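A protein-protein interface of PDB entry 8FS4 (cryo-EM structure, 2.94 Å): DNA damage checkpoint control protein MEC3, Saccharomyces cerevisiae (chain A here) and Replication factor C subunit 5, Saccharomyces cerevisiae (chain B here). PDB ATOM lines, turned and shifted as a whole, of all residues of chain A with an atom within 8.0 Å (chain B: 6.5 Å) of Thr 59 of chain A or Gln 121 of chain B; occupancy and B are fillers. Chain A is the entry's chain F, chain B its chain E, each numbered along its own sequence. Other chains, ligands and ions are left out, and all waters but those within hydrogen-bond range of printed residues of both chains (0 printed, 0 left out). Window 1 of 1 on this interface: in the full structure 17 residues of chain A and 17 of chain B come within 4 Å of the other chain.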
ATOM      1  N   ARG A  30      26.195 -10.787  15.256  1.00  0.00           N
ATOM      2  CA  ARG A  30      25.088 -10.732  16.202  1.00  0.00           C
ATOM      3  C   ARG A  30      24.778  -9.276  16.512  1.00  0.00           C
ATOM      4  O   ARG A  30      25.535  -8.367  16.160  1.00  0.00           O
ATOM      5  CB  ARG A  30      25.412 -11.506  17.483  1.00  0.00           C
ATOM      6  CG  ARG A  30      26.558 -10.907  18.289  1.00  0.00           C
ATOM      7  CD  ARG A  30      27.037 -11.846  19.386  1.00  0.00           C
ATOM      8  NE  ARG A  30      27.216 -13.214  18.912  1.00  0.00           N
ATOM      9  CZ  ARG A  30      28.330 -13.685  18.370  1.00  0.00           C
ATOM     10  NH1 ARG A  30      29.403 -12.925  18.216  1.00  0.00           N
ATOM     11  NH2 ARG A  30      28.369 -14.952  17.967  1.00  0.00           N
ATOM     12  N   PRO A  48      29.540 -14.036  22.589  1.00  0.00           N
ATOM     13  CA  PRO A  48      28.209 -14.357  23.120  1.00  0.00           C
ATOM     14  C   PRO A  48      28.079 -14.176  24.622  1.00  0.00           C
ATOM     15  O   PRO A  48      26.949 -14.179  25.130  1.00  0.00           O
ATOM     16  CB  PRO A  48      28.035 -15.827  22.730  1.00  0.00           C
ATOM     17  CG  PRO A  48      29.421 -16.374  22.784  1.00  0.00           C
ATOM     18  CD  PRO A  48      30.344 -15.252  22.364  1.00  0.00           C
ATOM     19  N   LYS A  49      29.188 -14.020  25.347  1.00  0.00           N
ATOM     20  CA  LYS A  49      29.162 -13.877  26.802  1.00  0.00           C
ATOM     21  C   LYS A  49      29.243 -12.392  27.142  1.00  0.00           C
ATOM     22  O   LYS A  49      30.299 -11.866  27.490  1.00  0.00           O
ATOM     23  CB  LYS A  49      30.303 -14.664  27.437  1.00  0.00           C
ATOM     24  CG  LYS A  49      30.138 -16.172  27.376  1.00  0.00           C
ATOM     25  CD  LYS A  49      31.302 -16.869  28.065  1.00  0.00           C
ATOM     26  CE  LYS A  49      31.424 -18.326  27.647  1.00  0.00           C
ATOM     27  NZ  LYS A  49      30.794 -19.244  28.638  1.00  0.00           N
ATOM     28  N   SER A  54      24.100  -9.106  24.523  1.00  0.00           N
ATOM     29  CA  SER A  54      23.642 -10.398  24.027  1.00  0.00           C
ATOM     30  C   SER A  54      22.820 -11.121  25.089  1.00  0.00           C
ATOM     31  O   SER A  54      23.364 -11.845  25.923  1.00  0.00           O
ATOM     32  CB  SER A  54      24.832 -11.262  23.604  1.00  0.00           C
ATOM     33  OG  SER A  54      24.400 -12.499  23.063  1.00  0.00           O
ATOM     34  N   ASN A  56      19.553 -12.575  24.030  1.00  0.00           N
ATOM     35  CA  ASN A  56      18.484 -13.193  23.244  1.00  0.00           C
ATOM     36  C   ASN A  56      19.046 -14.456  22.598  1.00  0.00           C
ATOM     37  O   ASN A  56      19.575 -14.411  21.485  1.00  0.00           O
ATOM     38  CB  ASN A  56      17.942 -12.225  22.198  1.00  0.00           C
ATOM     39  CG  ASN A  56      17.305 -10.996  22.814  1.00  0.00           C
ATOM     40  OD1 ASN A  56      16.992 -10.975  24.004  1.00  0.00           O
ATOM     41  ND2 ASN A  56      17.112  -9.963  22.003  1.00  0.00           N
ATOM     42  N   ASN A  57      18.925 -15.580  23.300  1.00  0.00           N
ATOM     43  CA  ASN A  57      19.331 -16.886  22.787  1.00  0.00           C
ATOM     44  C   ASN A  57      20.749 -16.835  22.210  1.00  0.00           C
ATOM     45  O   ASN A  57      20.980 -17.044  21.019  1.00  0.00           O
ATOM     46  CB  ASN A  57      18.335 -17.392  21.739  1.00  0.00           C
ATOM     47  CG  ASN A  57      16.914 -17.462  22.266  1.00  0.00           C
ATOM     48  OD1 ASN A  57      16.377 -18.545  22.494  1.00  0.00           O
ATOM     49  ND2 ASN A  57      16.298 -16.306  22.457  1.00  0.00           N
ATOM     50  N   GLY A  58      21.700 -16.545  23.099  1.00  0.00           N
ATOM     51  CA  GLY A  58      23.095 -16.571  22.691  1.00  0.00           C
ATOM     52  C   GLY A  58      23.509 -17.936  22.178  1.00  0.00           C
ATOM     53  O   GLY A  58      24.106 -18.059  21.106  1.00  0.00           O
ATOM     54  N   THR A  59      23.183 -18.984  22.936  1.00  0.00           N
ATOM     55  CA  THR A  59      23.335 -20.361  22.482  1.00  0.00           C
ATOM     56  C   THR A  59      22.070 -21.170  22.748  1.00  0.00           C
ATOM     57  O   THR A  59      22.124 -22.404  22.782  1.00  0.00           O
ATOM     58  CB  THR A  59      24.541 -21.028  23.152  1.00  0.00           C
ATOM     59  OG1 THR A  59      24.326 -21.103  24.566  1.00  0.00           O
ATOM     60  CG2 THR A  59      25.819 -20.244  22.872  1.00  0.00           C
ATOM     61  N   ILE A  60      20.934 -20.500  22.936  1.00  0.00           N
ATOM     62  CA  ILE A  60      19.650 -21.162  23.159  1.00  0.00           C
ATOM     63  C   ILE A  60      19.081 -21.506  21.785  1.00  0.00           C
ATOM     64  O   ILE A  60      18.465 -20.663  21.133  1.00  0.00           O
ATOM     65  CB  ILE A  60      18.677 -20.288  23.951  1.00  0.00           C
ATOM     66  CG1 ILE A  60      19.359 -19.585  25.124  1.00  0.00           C
ATOM     67  CG2 ILE A  60      17.512 -21.126  24.458  1.00  0.00           C
ATOM     68  CD1 ILE A  60      18.448 -18.568  25.775  1.00  0.00           C
ATOM     69  N   LEU A  61      19.318 -22.733  21.329  1.00  0.00           N
ATOM     70  CA  LEU A  61      18.765 -23.251  20.080  1.00  0.00           C
ATOM     71  C   LEU A  61      19.417 -22.635  18.852  1.00  0.00           C
ATOM     72  O   LEU A  61      19.255 -23.145  17.738  1.00  0.00           O
ATOM     73  CB  LEU A  61      17.266 -22.970  19.965  1.00  0.00           C
ATOM     74  CG  LEU A  61      16.211 -23.723  20.751  1.00  0.00           C
ATOM     75  CD1 LEU A  61      15.143 -22.772  21.211  1.00  0.00           C
ATOM     76  CD2 LEU A  61      15.639 -24.707  19.837  1.00  0.00           C
ATOM     77  N   ARG A  62      20.170 -21.553  19.040  1.00  0.00           N
ATOM     78  CA  ARG A  62      20.830 -20.903  17.921  1.00  0.00           C
ATOM     79  C   ARG A  62      22.176 -21.563  17.669  1.00  0.00           C
ATOM     80  O   ARG A  62      22.552 -21.840  16.526  1.00  0.00           O
ATOM     81  CB  ARG A  62      20.993 -19.406  18.209  1.00  0.00           C
ATOM     82  CG  ARG A  62      19.674 -18.659  18.375  1.00  0.00           C
ATOM     83  CD  ARG A  62      19.797 -17.203  17.917  1.00  0.00           C
ATOM     84  NE  ARG A  62      18.711 -16.333  18.364  1.00  0.00           N
ATOM     85  CZ  ARG A  62      17.414 -16.561  18.188  1.00  0.00           C
ATOM     86  NH1 ARG A  62      16.973 -17.617  17.523  1.00  0.00           N
ATOM     87  NH2 ARG A  62      16.533 -15.695  18.680  1.00  0.00           N
ATOM     88  N   GLY A  63      22.898 -21.845  18.748  1.00  0.00           N
ATOM     89  CA  GLY A  63      24.239 -22.367  18.629  1.00  0.00           C
ATOM     90  C   GLY A  63      25.261 -21.326  18.254  1.00  0.00           C
ATOM     91  O   GLY A  63      26.375 -21.680  17.856  1.00  0.00           O
ATOM     92  N   ASP A  64      24.916 -20.045  18.365  1.00  0.00           N
ATOM     93  CA  ASP A  64      25.829 -18.959  18.023  1.00  0.00           C
ATOM     94  C   ASP A  64      26.858 -18.840  19.138  1.00  0.00           C
ATOM     95  O   ASP A  64      26.625 -18.176  20.149  1.00  0.00           O
ATOM     96  CB  ASP A  64      25.064 -17.655  17.829  1.00  0.00           C
ATOM     97  CG  ASP A  64      23.954 -17.778  16.803  1.00  0.00           C
ATOM     98  OD1 ASP A  64      23.923 -18.792  16.077  1.00  0.00           O
ATOM     99  OD2 ASP A  64      23.113 -16.858  16.723  1.00  0.00           O
ATOM    100  N   THR A  65      28.006 -19.489  18.951  1.00  0.00           N
ATOM    101  CA  THR A  65      29.059 -19.527  19.956  1.00  0.00           C
ATOM    102  C   THR A  65      30.325 -18.801  19.534  1.00  0.00           C
ATOM    103  O   THR A  65      31.092 -18.373  20.399  1.00  0.00           O
ATOM    104  CB  THR A  65      29.408 -20.983  20.295  1.00  0.00           C
ATOM    105  OG1 THR A  65      28.286 -21.610  20.928  1.00  0.00           O
ATOM    106  CG2 THR A  65      30.610 -21.059  21.224  1.00  0.00           C
ATOM    107  N   GLY A  66      30.559 -18.643  18.233  1.00  0.00           N
ATOM    108  CA  GLY A  66      31.771 -18.010  17.752  1.00  0.00           C
ATOM    109  C   GLY A  66      31.985 -16.624  18.325  1.00  0.00           C
ATOM    110  O   GLY A  66      31.054 -15.813  18.374  1.00  0.00           O
ATOM    111  N   ALA A 469      34.057 -22.552  17.430  1.00  0.00           N
ATOM    112  CA  ALA A 469      34.057 -23.858  18.128  1.00  0.00           C
ATOM    113  C   ALA A 469      33.466 -24.938  17.217  1.00  0.00           C
ATOM    114  O   ALA A 469      32.684 -24.587  16.311  1.00  0.00           O
ATOM    115  CB  ALA A 469      33.269 -23.746  19.408  1.00  0.00           C
ATOM    116  N   ARG A 470      33.813 -26.202  17.468  1.00  0.00           N
ATOM    117  CA  ARG A 470      33.275 -27.328  16.662  1.00  0.00           C
ATOM    118  C   ARG A 470      31.747 -27.329  16.752  1.00  0.00           C
ATOM    119  O   ARG A 470      31.224 -27.220  17.875  1.00  0.00           O
ATOM    120  CB  ARG A 470      33.848 -28.650  17.176  1.00  0.00           C
ATOM    121  CG  ARG A 470      34.089 -28.668  18.679  1.00  0.00           C
ATOM    122  CD  ARG A 470      34.374 -30.049  19.232  1.00  0.00           C
ATOM    123  NE  ARG A 470      33.172 -30.866  19.306  1.00  0.00           N
ATOM    124  CZ  ARG A 470      33.134 -32.103  19.786  1.00  0.00           C
ATOM    125  NH1 ARG A 470      34.258 -32.742  20.054  1.00  0.00           N
ATOM    126  NH2 ARG A 470      31.971 -32.696  19.996  1.00  0.00           N
ATOM    127  N   SER A 471      31.071 -27.460  15.607  1.00  0.00           N
ATOM    128  CA  SER A 471      29.592 -27.583  15.558  1.00  0.00           C
ATOM    129  C   SER A 471      29.205 -29.062  15.541  1.00  0.00           C
ATOM    130  O   SER A 471      28.008 -29.347  15.361  1.00  0.00           O
ATOM    131  CB  SER A 471      29.028 -26.866  14.367  1.00  0.00           C
ATOM    132  OG  SER A 471      29.375 -25.490  14.400  1.00  0.00           O
ATOM    133  N   PRO B  91      18.359 -18.417  29.364  1.00  0.00           N
ATOM    134  CA  PRO B  91      19.763 -18.633  28.977  1.00  0.00           C
ATOM    135  C   PRO B  91      20.318 -19.985  29.393  1.00  0.00           C
ATOM    136  O   PRO B  91      21.375 -20.378  28.889  1.00  0.00           O
ATOM    137  CB  PRO B  91      20.507 -17.482  29.672  1.00  0.00           C
ATOM    138  CG  PRO B  91      19.526 -16.875  30.631  1.00  0.00           C
ATOM    139  CD  PRO B  91      18.177 -17.138  30.068  1.00  0.00           C
ATOM    140  N   GLN B 118      20.430 -32.482  19.542  1.00  0.00           N
ATOM    141  CA  GLN B 118      21.561 -32.765  18.668  1.00  0.00           C
ATOM    142  C   GLN B 118      22.709 -31.788  18.881  1.00  0.00           C
ATOM    143  O   GLN B 118      23.874 -32.169  18.727  1.00  0.00           O
ATOM    144  CB  GLN B 118      21.111 -32.735  17.206  1.00  0.00           C
ATOM    145  CG  GLN B 118      20.578 -34.067  16.700  1.00  0.00           C
ATOM    146  CD  GLN B 118      19.826 -33.934  15.391  1.00  0.00           C
ATOM    147  OE1 GLN B 118      19.723 -32.846  14.827  1.00  0.00           O
ATOM    148  NE2 GLN B 118      19.296 -35.047  14.900  1.00  0.00           N
ATOM    149  N   MET B 119      22.413 -30.539  19.234  1.00  0.00           N
ATOM    150  CA  MET B 119      23.464 -29.557  19.466  1.00  0.00           C
ATOM    151  C   MET B 119      24.178 -29.860  20.777  1.00  0.00           C
ATOM    152  O   MET B 119      23.539 -30.069  21.813  1.00  0.00           O
ATOM    153  CB  MET B 119      22.874 -28.149  19.493  1.00  0.00           C
ATOM    154  CG  MET B 119      22.107 -27.787  18.226  1.00  0.00           C
ATOM    155  SD  MET B 119      21.484 -26.091  18.132  1.00  0.00           S
ATOM    156  CE  MET B 119      22.489 -25.238  19.344  1.00  0.00           C
ATOM    157  N   GLU B 120      25.512 -29.880  20.732  1.00  0.00           N
ATOM    158  CA  GLU B 120      26.293 -30.321  21.884  1.00  0.00           C
ATOM    159  C   GLU B 120      26.373 -29.256  22.970  1.00  0.00           C
ATOM    160  O   GLU B 120      26.460 -29.588  24.157  1.00  0.00           O
ATOM    161  CB  GLU B 120      27.698 -30.724  21.439  1.00  0.00           C
ATOM    162  CG  GLU B 120      28.393 -31.663  22.409  1.00  0.00           C
ATOM    163  CD  GLU B 120      28.279 -33.117  22.000  1.00  0.00           C
ATOM    164  OE1 GLU B 120      27.948 -33.955  22.866  1.00  0.00           O
ATOM    165  OE2 GLU B 120      28.523 -33.424  20.815  1.00  0.00           O
ATOM    166  N   GLN B 121      26.357 -27.978  22.594  1.00  0.00           N
ATOM    167  CA  GLN B 121      26.458 -26.813  23.469  1.00  0.00           C
ATOM    168  C   GLN B 121      27.899 -26.536  23.884  1.00  0.00           C
ATOM    169  O   GLN B 121      28.135 -25.581  24.621  1.00  0.00           O
ATOM    170  CB  GLN B 121      25.585 -26.933  24.734  1.00  0.00           C
ATOM    171  CG  GLN B 121      25.272 -25.625  25.471  1.00  0.00           C
ATOM    172  CD  GLN B 121      25.191 -24.412  24.566  1.00  0.00           C
ATOM    173  OE1 GLN B 121      24.497 -24.424  23.549  1.00  0.00           O
ATOM    174  NE2 GLN B 121      25.907 -23.356  24.931  1.00  0.00           N
ATOM    175  N   VAL B 122      28.867 -27.338  23.435  1.00  0.00           N
ATOM    176  CA  VAL B 122      30.258 -27.118  23.810  1.00  0.00           C
ATOM    177  C   VAL B 122      30.681 -25.721  23.388  1.00  0.00           C
ATOM    178  O   VAL B 122      30.479 -25.312  22.239  1.00  0.00           O
ATOM    179  CB  VAL B 122      31.158 -28.196  23.181  1.00  0.00           C
ATOM    180  CG1 VAL B 122      31.090 -28.132  21.666  1.00  0.00           C
ATOM    181  CG2 VAL B 122      32.598 -28.049  23.664  1.00  0.00           C
ATOM    182  N   ASP B 123      31.273 -24.983  24.324  1.00  0.00           N
ATOM    183  CA  ASP B 123      31.771 -23.627  24.100  1.00  0.00           C
ATOM    184  C   ASP B 123      33.242 -23.617  24.501  1.00  0.00           C
ATOM    185  O   ASP B 123      33.585 -23.340  25.653  1.00  0.00           O
ATOM    186  CB  ASP B 123      30.956 -22.598  24.892  1.00  0.00           C
ATOM    187  CG  ASP B 123      31.291 -21.166  24.512  1.00  0.00           C
ATOM    188  OD1 ASP B 123      32.448 -20.904  24.123  1.00  0.00           O
ATOM    189  OD2 ASP B 123      30.393 -20.302  24.598  1.00  0.00           O
ATOM    190  N   PHE B 124      34.110 -23.925  23.539  1.00  0.00           N
ATOM    191  CA  PHE B 124      35.557 -23.953  23.752  1.00  0.00           C
ATOM    192  C   PHE B 124      35.921 -24.936  24.864  1.00  0.00           C
ATOM    193  O   PHE B 124      36.434 -24.570  25.924  1.00  0.00           O
ATOM    194  CB  PHE B 124      36.090 -22.547  24.040  1.00  0.00           C
ATOM    195  CG  PHE B 124      35.960 -21.608  22.875  1.00  0.00           C
ATOM    196  CD1 PHE B 124      35.412 -22.033  21.681  1.00  0.00           C
ATOM    197  CD2 PHE B 124      36.396 -20.308  22.961  1.00  0.00           C
ATOM    198  CE1 PHE B 124      35.296 -21.181  20.611  1.00  0.00           C
ATOM    199  CE2 PHE B 124      36.284 -19.464  21.877  1.00  0.00           C
ATOM    200  CZ  PHE B 124      35.725 -19.898  20.713  1.00  0.00           C
ATOM    201  N   ASP B 126      33.835 -26.833  26.666  1.00  0.00           N
ATOM    202  CA  ASP B 126      32.906 -26.669  27.786  1.00  0.00           C
ATOM    203  C   ASP B 126      33.389 -27.319  29.077  1.00  0.00           C
ATOM    204  O   ASP B 126      33.642 -28.523  29.117  1.00  0.00           O
ATOM    205  CB  ASP B 126      31.543 -27.259  27.422  1.00  0.00           C
ATOM    206  CG  ASP B 126      30.473 -26.203  27.217  1.00  0.00           C
ATOM    207  OD1 ASP B 126      30.812 -25.005  27.123  1.00  0.00           O
ATOM    208  OD2 ASP B 126      29.285 -26.579  27.147  1.00  0.00           O
ATOM    209  N   HIS B 133      25.440 -24.553  31.798  1.00  0.00           N
ATOM    210  CA  HIS B 133      25.605 -24.270  30.370  1.00  0.00           C
ATOM    211  C   HIS B 133      26.485 -25.320  29.690  1.00  0.00           C
ATOM    212  O   HIS B 133      27.261 -25.016  28.782  1.00  0.00           O
ATOM    213  CB  HIS B 133      26.153 -22.854  30.139  1.00  0.00           C
ATOM    214  CG  HIS B 133      27.319 -22.495  31.008  1.00  0.00           C
ATOM    215  ND1 HIS B 133      27.171 -22.051  32.305  1.00  0.00           N
ATOM    216  CD2 HIS B 133      28.651 -22.513  30.767  1.00  0.00           C
ATOM    217  CE1 HIS B 133      28.362 -21.814  32.826  1.00  0.00           C
ATOM    218  NE2 HIS B 133      29.277 -22.086  31.913  1.00  0.00           N
ATOM    219  N   ARG B 134      26.367 -26.573  30.140  1.00  0.00           N
ATOM    220  CA  ARG B 134      26.992 -27.702  29.451  1.00  0.00           C
ATOM    221  C   ARG B 134      25.927 -28.633  28.891  1.00  0.00           C
ATOM    222  O   ARG B 134      25.881 -28.840  27.677  1.00  0.00           O
ATOM    223  CB  ARG B 134      27.936 -28.454  30.391  1.00  0.00           C
ATOM    224  CG  ARG B 134      28.346 -29.836  29.880  1.00  0.00           C
ATOM    225  CD  ARG B 134      29.000 -29.744  28.508  1.00  0.00           C
ATOM    226  NE  ARG B 134      29.373 -31.045  27.965  1.00  0.00           N
ATOM    227  CZ  ARG B 134      28.925 -31.552  26.821  1.00  0.00           C
ATOM    228  NH1 ARG B 134      28.052 -30.904  26.065  1.00  0.00           N
ATOM    229  NH2 ARG B 134      29.365 -32.742  26.424  1.00  0.00           N
ATOM    230  N   TYR B 135      25.065 -29.195  29.731  1.00  0.00           N
ATOM    231  CA  TYR B 135      23.864 -29.856  29.259  1.00  0.00           C
ATOM    232  C   TYR B 135      22.698 -28.880  29.357  1.00  0.00           C
ATOM    233  O   TYR B 135      22.801 -27.807  29.955  1.00  0.00           O
ATOM    234  CB  TYR B 135      23.595 -31.150  30.041  1.00  0.00           C
ATOM    235  CG  TYR B 135      23.329 -31.014  31.531  1.00  0.00           C
ATOM    236  CD1 TYR B 135      22.297 -30.223  32.017  1.00  0.00           C
ATOM    237  CD2 TYR B 135      24.100 -31.708  32.451  1.00  0.00           C
ATOM    238  CE1 TYR B 135      22.058 -30.115  33.368  1.00  0.00           C
ATOM    239  CE2 TYR B 135      23.866 -31.605  33.805  1.00  0.00           C
ATOM    240  CZ  TYR B 135      22.843 -30.808  34.256  1.00  0.00           C
ATOM    241  OH  TYR B 135      22.605 -30.699  35.604  1.00  0.00           O
ATOM    242  N   LYS B 136      21.580 -29.256  28.756  1.00  0.00           N
ATOM    243  CA  LYS B 136      20.424 -28.383  28.675  1.00  0.00           C
ATOM    244  C   LYS B 136      19.233 -29.020  29.371  1.00  0.00           C
ATOM    245  O   LYS B 136      19.063 -30.241  29.357  1.00  0.00           O
ATOM    246  CB  LYS B 136      20.070 -28.075  27.225  1.00  0.00           C
ATOM    247  CG  LYS B 136      20.700 -26.799  26.710  1.00  0.00           C
ATOM    248  CD  LYS B 136      19.806 -26.104  25.704  1.00  0.00           C
ATOM    249  CE  LYS B 136      19.974 -24.600  25.772  1.00  0.00           C
ATOM    250  NZ  LYS B 136      18.852 -23.900  25.104  1.00  0.00           N
ATOM    251  N   ASN B 164      23.957 -33.978  26.372  1.00  0.00           N
ATOM    252  CA  ASN B 164      23.858 -32.538  26.188  1.00  0.00           C
ATOM    253  C   ASN B 164      22.457 -31.994  26.422  1.00  0.00           C
ATOM    254  O   ASN B 164      22.222 -30.809  26.171  1.00  0.00           O
ATOM    255  CB  ASN B 164      24.334 -32.156  24.782  1.00  0.00           C
ATOM    256  CG  ASN B 164      23.240 -32.258  23.742  1.00  0.00           C
ATOM    257  OD1 ASN B 164      22.331 -31.430  23.692  1.00  0.00           O
ATOM    258  ND2 ASN B 164      23.327 -33.276  22.894  1.00  0.00           N
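The backbone NH of Asp 123 of chain B is in hydrogen-bond range of the side-chain carboxylate of Asp 126 of chain B, at 2.8 Å. The backbone carbonyl oxygen (O) of Asn 164 of chain B sits at hydrogen-bond distance from the backbone NH (N) of Lys 136 of chain B (3.1 Å). The side-chain amide oxygen of Asn 57 of chain A lies close to the backbone carbonyl oxygen of Ile 60 of chain A (3.3 Å). NH1 of Arg 134 of chain B sits at hydrogen-bond distance from O of Glu 120 of chain B (2.8 Å). O of Met 119 of chain B sits close to OD1 of Asn 164 of chain B, 2.6 Å away.
The side-chain amide nitrogen (NE2) of Gln 121 of chain B sits at hydrogen-bond distance from the side-chain hydroxyl (OG1) of Thr 59 of chain A, 2.8 Å away. The guanidinium group (NH2) of Arg 470 of chain A lies within salt-bridge range of the side-chain carboxylate (OE2) of Glu 120 of chain B (3.6 Å). O of Leu 61 of chain A sits close to SD of Met 119 of chain B, 3.7 Å away.
Hydrophobic or aromatic side chains of chain B within 4 Å of the printed part of chain A: Met 119, Val 122 and Phe 124. Among the printed residues, 11 pairs touch across the chains. Among the printed residues, Asp or Glu carboxylates within 4 Å of a Lys or Arg side-chain nitrogen of the other chain: Arg 470 of chain A with Glu 120 of chain B (3.6 Å).
Thr 59 of chain A touches just one residue of chain B: Gln 121 (2.8 Å). Gln 121 of chain B touches just one residue of chain A: Thr 59. Printed residues of chain B within 4 Å of Ala 469 of chain A: Phe 124 (3.5 Å). Printed residues of chain B within 4 Å of Gly 63 of chain A: Met 119 (3.4 Å). Of the printed residues of chain A, Phe 124 of chain B touches Ala 469. Of the printed residues of chain B, Ile 60 of chain A touches Pro 91 and Lys 136. Of the printed residues of chain A, Pro 91 of chain B touches Ile 60 (3.5 Å). Asn 57 of chain A touches none of the printed residues of chain B. Arg 30 of chain A touches none of the printed residues of chain B. The nearest residue of chain B that does not touch Thr 59 of chain A is Lys 136 of chain B (4.3 Å).
Among the printed residues, pairs that only touch across the chains: Ile 60 of chain A with Lys 136 of chain B (3.1 Å), Thr 65 of chain A with Asp 123 of chain B (3.4 Å), Gly 63 of chain A with Met 119 of chain B (3.4 Å), Ile 60 of chain A with Pro 91 of chain B (3.5 Å), Ala 469 of chain A with Phe 124 of chain B (3.5 Å), Lys 49 of chain A with Asp 123 of chain B (3.8 Å), Arg 470 of chain A with Val 122 of chain B (3.9 Å) and Leu 61 of chain A with Lys 136 of chain B (3.98 Å).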
